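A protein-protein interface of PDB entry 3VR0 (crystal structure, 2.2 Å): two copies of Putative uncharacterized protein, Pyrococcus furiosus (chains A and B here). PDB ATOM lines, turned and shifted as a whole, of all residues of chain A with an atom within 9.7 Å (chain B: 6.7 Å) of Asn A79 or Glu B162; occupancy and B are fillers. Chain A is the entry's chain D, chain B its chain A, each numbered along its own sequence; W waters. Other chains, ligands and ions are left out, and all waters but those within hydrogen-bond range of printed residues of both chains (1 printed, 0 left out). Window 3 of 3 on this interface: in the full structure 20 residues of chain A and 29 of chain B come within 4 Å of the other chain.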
ATOM      1  N   LEU A  75     -12.688 -13.190   9.685  1.00  0.00           N
ATOM      2  CA  LEU A  75     -14.119 -13.134   9.386  1.00  0.00           C
ATOM      3  C   LEU A  75     -14.330 -12.668   7.945  1.00  0.00           C
ATOM      4  O   LEU A  75     -13.563 -11.859   7.411  1.00  0.00           O
ATOM      5  CB  LEU A  75     -14.810 -12.136  10.319  1.00  0.00           C
ATOM      6  CG  LEU A  75     -14.877 -12.484  11.816  1.00  0.00           C
ATOM      7  CD1 LEU A  75     -15.578 -11.384  12.565  1.00  0.00           C
ATOM      8  CD2 LEU A  75     -15.538 -13.840  12.108  1.00  0.00           C
ATOM      9  N   ILE A  76     -15.394 -13.171   7.332  1.00  0.00           N
ATOM     10  CA  ILE A  76     -15.825 -12.704   6.035  1.00  0.00           C
ATOM     11  C   ILE A  76     -16.543 -11.375   6.207  1.00  0.00           C
ATOM     12  O   ILE A  76     -17.518 -11.328   6.911  1.00  0.00           O
ATOM     13  CB  ILE A  76     -16.752 -13.723   5.419  1.00  0.00           C
ATOM     14  CG1 ILE A  76     -16.009 -15.064   5.237  1.00  0.00           C
ATOM     15  CG2 ILE A  76     -17.259 -13.232   4.033  1.00  0.00           C
ATOM     16  CD1 ILE A  76     -14.688 -14.986   4.339  1.00  0.00           C
ATOM     17  N   ARG A  77     -16.046 -10.284   5.614  1.00  0.00           N
ATOM     18  CA  ARG A  77     -16.773  -8.996   5.664  1.00  0.00           C
ATOM     19  C   ARG A  77     -17.642  -8.828   4.383  1.00  0.00           C
ATOM     20  O   ARG A  77     -17.893  -9.800   3.671  1.00  0.00           O
ATOM     21  CB  ARG A  77     -15.826  -7.782   5.836  1.00  0.00           C
ATOM     22  CG  ARG A  77     -14.725  -7.931   6.883  1.00  0.00           C
ATOM     23  CD  ARG A  77     -15.325  -8.083   8.255  1.00  0.00           C
ATOM     24  NE  ARG A  77     -14.369  -7.728   9.284  1.00  0.00           N
ATOM     25  CZ  ARG A  77     -14.576  -7.859  10.594  1.00  0.00           C
ATOM     26  NH1 ARG A  77     -15.736  -8.320  11.041  1.00  0.00           N
ATOM     27  NH2 ARG A  77     -13.613  -7.502  11.455  1.00  0.00           N
ATOM     28  N   LYS A  78     -18.095  -7.610   4.102  1.00  0.00           N
ATOM     29  CA  LYS A  78     -18.826  -7.327   2.846  1.00  0.00           C
ATOM     30  C   LYS A  78     -17.883  -7.470   1.673  1.00  0.00           C
ATOM     31  O   LYS A  78     -16.658  -7.229   1.803  1.00  0.00           O
ATOM     32  CB  LYS A  78     -19.406  -5.904   2.853  1.00  0.00           C
ATOM     33  CG  LYS A  78     -20.649  -5.748   3.731  1.00  0.00           C
ATOM     34  CD  LYS A  78     -20.939  -4.279   4.093  1.00  0.00           C
ATOM     35  CE  LYS A  78     -22.097  -4.147   5.124  1.00  0.00           C
ATOM     36  NZ  LYS A  78     -23.240  -5.140   4.967  1.00  0.00           N
ATOM     37  N   ASN A  79     -18.444  -7.887   0.539  1.00  0.00           N
ATOM     38  CA  ASN A  79     -17.752  -7.872  -0.717  1.00  0.00           C
ATOM     39  C   ASN A  79     -16.616  -8.954  -0.733  1.00  0.00           C
ATOM     40  O   ASN A  79     -15.585  -8.776  -1.392  1.00  0.00           O
ATOM     41  CB  ASN A  79     -17.221  -6.456  -1.011  1.00  0.00           C
ATOM     42  CG  ASN A  79     -18.355  -5.414  -1.251  1.00  0.00           C
ATOM     43  OD1 ASN A  79     -18.349  -4.295  -0.686  1.00  0.00           O
ATOM     44  ND2 ASN A  79     -19.323  -5.784  -2.082  1.00  0.00           N
ATOM     45  N   SER A  80     -16.849 -10.078  -0.029  1.00  0.00           N
ATOM     46  CA  SER A  80     -15.925 -11.233  -0.045  1.00  0.00           C
ATOM     47  C   SER A  80     -14.510 -10.864   0.473  1.00  0.00           C
ATOM     48  O   SER A  80     -13.536 -11.408   0.019  1.00  0.00           O
ATOM     49  CB  SER A  80     -15.825 -11.770  -1.482  1.00  0.00           C
ATOM     50  OG  SER A  80     -17.086 -12.166  -1.996  1.00  0.00           O
ATOM     51  N   VAL A  81     -14.434  -9.917   1.394  1.00  0.00           N
ATOM     52  CA  VAL A  81     -13.204  -9.457   1.996  1.00  0.00           C
ATOM     53  C   VAL A  81     -12.935 -10.194   3.351  1.00  0.00           C
ATOM     54  O   VAL A  81     -13.827 -10.320   4.148  1.00  0.00           O
ATOM     55  CB  VAL A  81     -13.259  -7.890   2.169  1.00  0.00           C
ATOM     56  CG1 VAL A  81     -12.056  -7.327   3.030  1.00  0.00           C
ATOM     57  CG2 VAL A  81     -13.239  -7.231   0.762  1.00  0.00           C
ATOM     58  N   VAL A  82     -11.736 -10.733   3.570  1.00  0.00           N
ATOM     59  CA  VAL A  82     -11.380 -11.278   4.904  1.00  0.00           C
ATOM     60  C   VAL A  82     -10.691 -10.237   5.759  1.00  0.00           C
ATOM     61  O   VAL A  82     -10.019  -9.361   5.244  1.00  0.00           O
ATOM     62  CB  VAL A  82     -10.471 -12.538   4.837  1.00  0.00           C
ATOM     63  CG1 VAL A  82     -11.118 -13.618   4.005  1.00  0.00           C
ATOM     64  CG2 VAL A  82      -9.098 -12.219   4.276  1.00  0.00           C
ATOM     65  N   ALA B 158     -12.305 -15.707  -1.243  1.00  0.00           N
ATOM     66  CA  ALA B 158     -12.373 -14.449  -0.501  1.00  0.00           C
ATOM     67  C   ALA B 158     -11.008 -13.806  -0.614  1.00  0.00           C
ATOM     68  O   ALA B 158     -10.063 -14.519  -0.845  1.00  0.00           O
ATOM     69  CB  ALA B 158     -12.762 -14.679   0.951  1.00  0.00           C
ATOM     70  N   VAL B 159     -10.912 -12.481  -0.481  1.00  0.00           N
ATOM     71  CA  VAL B 159      -9.685 -11.756  -0.742  1.00  0.00           C
ATOM     72  C   VAL B 159      -9.447 -10.776   0.375  1.00  0.00           C
ATOM     73  O   VAL B 159     -10.363 -10.501   1.129  1.00  0.00           O
ATOM     74  CB  VAL B 159      -9.699 -10.943  -2.101  1.00  0.00           C
ATOM     75  CG1 VAL B 159      -9.600 -11.841  -3.263  1.00  0.00           C
ATOM     76  CG2 VAL B 159     -10.968 -10.105  -2.224  1.00  0.00           C
ATOM     77  N   THR B 160      -8.229 -10.234   0.467  1.00  0.00           N
ATOM     78  CA  THR B 160      -7.897  -9.237   1.474  1.00  0.00           C
ATOM     79  C   THR B 160      -8.368  -7.833   1.160  1.00  0.00           C
ATOM     80  O   THR B 160      -8.514  -7.015   2.074  1.00  0.00           O
ATOM     81  CB  THR B 160      -6.385  -9.184   1.650  1.00  0.00           C
ATOM     82  OG1 THR B 160      -5.792  -9.078   0.350  1.00  0.00           O
ATOM     83  CG2 THR B 160      -5.861 -10.536   2.301  1.00  0.00           C
ATOM     84  N   HIS B 161      -8.606  -7.545  -0.119  1.00  0.00           N
ATOM     85  CA  HIS B 161      -8.933  -6.163  -0.589  1.00  0.00           C
ATOM     86  C   HIS B 161      -9.964  -6.261  -1.724  1.00  0.00           C
ATOM     87  O   HIS B 161      -9.768  -7.005  -2.675  1.00  0.00           O
ATOM     88  CB  HIS B 161      -7.679  -5.405  -1.101  1.00  0.00           C
ATOM     89  CG  HIS B 161      -6.544  -5.377  -0.109  1.00  0.00           C
ATOM     90  ND1 HIS B 161      -6.347  -4.331   0.780  1.00  0.00           N
ATOM     91  CD2 HIS B 161      -5.579  -6.285   0.167  1.00  0.00           C
ATOM     92  CE1 HIS B 161      -5.306  -4.596   1.552  1.00  0.00           C
ATOM     93  NE2 HIS B 161      -4.812  -5.767   1.189  1.00  0.00           N
ATOM     94  N   GLU B 162     -11.047  -5.502  -1.621  1.00  0.00           N
ATOM     95  CA  GLU B 162     -12.088  -5.545  -2.658  1.00  0.00           C
ATOM     96  C   GLU B 162     -11.546  -5.454  -4.097  1.00  0.00           C
ATOM     97  O   GLU B 162     -11.968  -6.206  -4.966  1.00  0.00           O
ATOM     98  CB  GLU B 162     -13.117  -4.457  -2.413  1.00  0.00           C
ATOM     99  CG  GLU B 162     -14.419  -4.833  -3.080  1.00  0.00           C
ATOM    100  CD  GLU B 162     -15.471  -3.704  -3.131  1.00  0.00           C
ATOM    101  OE1 GLU B 162     -15.394  -2.726  -2.327  1.00  0.00           O
ATOM    102  OE2 GLU B 162     -16.380  -3.839  -3.998  1.00  0.00           O
ATOM    103  N   ASP B 163     -10.562  -4.602  -4.352  1.00  0.00           N
ATOM    104  CA  ASP B 163     -10.122  -4.491  -5.726  1.00  0.00           C
ATOM    105  C   ASP B 163      -9.468  -5.743  -6.249  1.00  0.00           C
ATOM    106  O   ASP B 163      -9.165  -5.847  -7.422  1.00  0.00           O
ATOM    107  CB  ASP B 163      -9.375  -3.158  -6.034  1.00  0.00           C
ATOM    108  CG  ASP B 163      -8.100  -2.949  -5.205  1.00  0.00           C
ATOM    109  OD1 ASP B 163      -7.748  -1.736  -4.970  1.00  0.00           O
ATOM    110  OD2 ASP B 163      -7.446  -3.959  -4.814  1.00  0.00           O
ATOM    111  N   LEU B 164      -9.305  -6.751  -5.390  1.00  0.00           N
ATOM    112  CA  LEU B 164      -8.672  -7.991  -5.860  1.00  0.00           C
ATOM    113  C   LEU B 164      -9.698  -8.948  -6.463  1.00  0.00           C
ATOM    114  O   LEU B 164      -9.340  -9.927  -7.150  1.00  0.00           O
ATOM    115  CB  LEU B 164      -7.893  -8.681  -4.708  1.00  0.00           C
ATOM    116  CG  LEU B 164      -6.617  -7.975  -4.244  1.00  0.00           C
ATOM    117  CD1 LEU B 164      -6.043  -8.730  -3.057  1.00  0.00           C
ATOM    118  CD2 LEU B 164      -5.633  -7.981  -5.429  1.00  0.00           C
ATOM    119  N   ILE B 165     -10.971  -8.695  -6.220  1.00  0.00           N
ATOM    120  CA  ILE B 165     -11.967  -9.610  -6.844  1.00  0.00           C
ATOM    121  C   ILE B 165     -11.779  -9.708  -8.374  1.00  0.00           C
ATOM    122  O   ILE B 165     -11.627 -10.816  -8.924  1.00  0.00           O
ATOM    123  CB  ILE B 165     -13.424  -9.237  -6.486  1.00  0.00           C
ATOM    124  CG1 ILE B 165     -13.629  -9.304  -4.974  1.00  0.00           C
ATOM    125  CG2 ILE B 165     -14.451 -10.193  -7.234  1.00  0.00           C
ATOM    126  CD1 ILE B 165     -14.865  -8.625  -4.505  1.00  0.00           C
ATOM    127  N   GLU B 166     -11.728  -8.549  -9.051  1.00  0.00           N
ATOM    128  CA  GLU B 166     -11.637  -8.514 -10.535  1.00  0.00           C
ATOM    129  C   GLU B 166     -10.331  -9.072 -10.940  1.00  0.00           C
ATOM    130  O   GLU B 166     -10.202  -9.801 -11.953  1.00  0.00           O
ATOM    131  CB  GLU B 166     -11.749  -7.072 -11.069  1.00  0.00           C
ATOM    132  CG  GLU B 166     -13.202  -6.588 -11.082  1.00  0.00           C
ATOM    133  CD  GLU B 166     -14.134  -7.529 -11.918  1.00  0.00           C
ATOM    134  OE1 GLU B 166     -13.672  -8.088 -12.961  1.00  0.00           O
ATOM    135  OE2 GLU B 166     -15.315  -7.727 -11.519  1.00  0.00           O
ATOM    136  N   TYR B 167      -9.326  -8.730 -10.139  1.00  0.00           N
ATOM    137  CA  TYR B 167      -7.986  -9.220 -10.422  1.00  0.00           C
ATOM    138  C   TYR B 167      -7.922 -10.740 -10.520  1.00  0.00           C
ATOM    139  O   TYR B 167      -7.429 -11.265 -11.496  1.00  0.00           O
ATOM    140  CB  TYR B 167      -6.995  -8.679  -9.364  1.00  0.00           C
ATOM    141  CG  TYR B 167      -5.567  -9.139  -9.584  1.00  0.00           C
ATOM    142  CD1 TYR B 167      -4.815  -8.654 -10.658  1.00  0.00           C
ATOM    143  CD2 TYR B 167      -4.966 -10.070  -8.709  1.00  0.00           C
ATOM    144  CE1 TYR B 167      -3.502  -9.057 -10.855  1.00  0.00           C
ATOM    145  CE2 TYR B 167      -3.657 -10.491  -8.906  1.00  0.00           C
ATOM    146  CZ  TYR B 167      -2.938  -9.971  -9.976  1.00  0.00           C
ATOM    147  OH  TYR B 167      -1.655 -10.391 -10.194  1.00  0.00           O
ATOM    148  N   TRP B 181     -17.719 -16.449  -5.224  1.00  0.00           N
ATOM    149  CA  TRP B 181     -17.313 -15.350  -4.373  1.00  0.00           C
ATOM    150  C   TRP B 181     -18.186 -15.251  -3.130  1.00  0.00           C
ATOM    151  O   TRP B 181     -19.342 -14.769  -3.172  1.00  0.00           O
ATOM    152  CB  TRP B 181     -17.229 -14.038  -5.171  1.00  0.00           C
ATOM    153  CG  TRP B 181     -16.150 -14.209  -6.162  1.00  0.00           C
ATOM    154  CD1 TRP B 181     -16.252 -14.793  -7.404  1.00  0.00           C
ATOM    155  CD2 TRP B 181     -14.756 -13.935  -5.954  1.00  0.00           C
ATOM    156  NE1 TRP B 181     -15.007 -14.861  -7.989  1.00  0.00           N
ATOM    157  CE2 TRP B 181     -14.074 -14.344  -7.119  1.00  0.00           C
ATOM    158  CE3 TRP B 181     -14.019 -13.385  -4.888  1.00  0.00           C
ATOM    159  CZ2 TRP B 181     -12.685 -14.216  -7.258  1.00  0.00           C
ATOM    160  CZ3 TRP B 181     -12.633 -13.243  -5.032  1.00  0.00           C
ATOM    161  CH2 TRP B 181     -11.991 -13.661  -6.211  1.00  0.00           C
ATOM    162  N   ARG B 182     -17.613 -15.699  -2.015  1.00  0.00           N
ATOM    163  CA  ARG B 182     -18.311 -15.806  -0.737  1.00  0.00           C
ATOM    164  C   ARG B 182     -19.048 -14.568  -0.312  1.00  0.00           C
ATOM    165  O   ARG B 182     -18.479 -13.470  -0.312  1.00  0.00           O
ATOM    166  CB  ARG B 182     -17.298 -16.095   0.371  1.00  0.00           C
ATOM    167  CG  ARG B 182     -16.759 -17.478   0.287  1.00  0.00           C
ATOM    168  CD  ARG B 182     -15.771 -17.694   1.364  1.00  0.00           C
ATOM    169  NE  ARG B 182     -16.413 -17.864   2.658  1.00  0.00           N
ATOM    170  CZ  ARG B 182     -15.846 -18.583   3.617  1.00  0.00           C
ATOM    171  NH1 ARG B 182     -14.660 -19.143   3.382  1.00  0.00           N
ATOM    172  NH2 ARG B 182     -16.441 -18.737   4.792  1.00  0.00           N
ATOM    173  N   GLU B 183     -20.281 -14.746   0.148  1.00  0.00           N
ATOM    174  CA  GLU B 183     -21.072 -13.634   0.671  1.00  0.00           C
ATOM    175  C   GLU B 183     -21.622 -13.922   2.064  1.00  0.00           C
ATOM    176  O   GLU B 183     -22.421 -13.138   2.599  1.00  0.00           O
ATOM    177  CB  GLU B 183     -22.218 -13.283  -0.287  1.00  0.00           C
ATOM    178  CG  GLU B 183     -21.774 -13.214  -1.740  1.00  0.00           C
ATOM    179  CD  GLU B 183     -22.885 -12.767  -2.689  1.00  0.00           C
ATOM    180  OE1 GLU B 183     -23.729 -11.916  -2.288  1.00  0.00           O
ATOM    181  OE2 GLU B 183     -22.885 -13.258  -3.853  1.00  0.00           O
HETATM  182  O   HOH W   1     -19.132 -11.023   1.523  1.00  0.00           O
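Of the printed residues of chain B, Asn A79 touches Glu B162 and Ile B165.
Glu B162 touches two residues of chain A.
No residue of chain A comes within 4 Å of Asp B163.
Of the printed residues of chain B, Val A82 touches Ala B158 and Val B159.
Of the printed residues of chain A, Ile B165 touches Asn A79 (3.2 Å).
Of the printed residues of chain A, Trp B181 touches Ser A80 (3.5 Å).
Leu A75 touches none of the printed residues of chain B.
Glu B183 touches none of the printed residues of chain A.
The nearest printed residue of chain A that does not touch Ala B158 is Val A81 (5.1 Å).
O of Ser A80 lies within hydrogen-bond range of N of Val B159 (2.9 Å).
O of Val B159 lies within hydrogen-bond range of N of Val A82, 2.8 Å away.
OG of Ser A80 lies within hydrogen-bond range of O of Arg B182, 2.5 Å away.
Hydrophobic or aromatic side chains of chain B within 4 Å of the printed part of chain A: Ala B158, Val B159, Ile B165 and Trp B181.
Hydrophobic or aromatic side chains of chain A within 4 Å of the printed part of chain B: Ile A76, Val A81 and Val A82.
Water W1 lies within hydrogen-bond range of the backbone carbonyl oxygen (O) of Arg A77 (2.8 Å), the backbone NH (N) of Ser A80 (2.9 Å), the backbone carbonyl oxygen (O) of Arg B182 (3.1 Å) and the backbone NH (N) of Asn A79 (3.4 Å).
No position is printed for both chains.
Of the 13 pairs that touch across the chains among the printed residues, none has its exchanged pair printed and touching as well.
Ile A76 touches Ala B158 (CD1 to CB, 3.9 Å).
Ile A76 touches Arg B182.
Asn A79 touches Glu B162 (OD1 to OE1, 3.7 Å).
Asn A79 touches Ile B165.
Ala B158 touches Ser A80.
Trp B181 touches Ser A80 (C to OG, 3.5 Å).
O of Val B159 touches CA of Val A81, at 3.1 Å.
Val A81 touches Thr B160 (CG1 to O, 3.7 Å).
CG2 of Val A81 touches N of Glu B162 (3.7 Å).
CB of Ala B158 touches CG1 of Val A82, at 3.6 Å.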
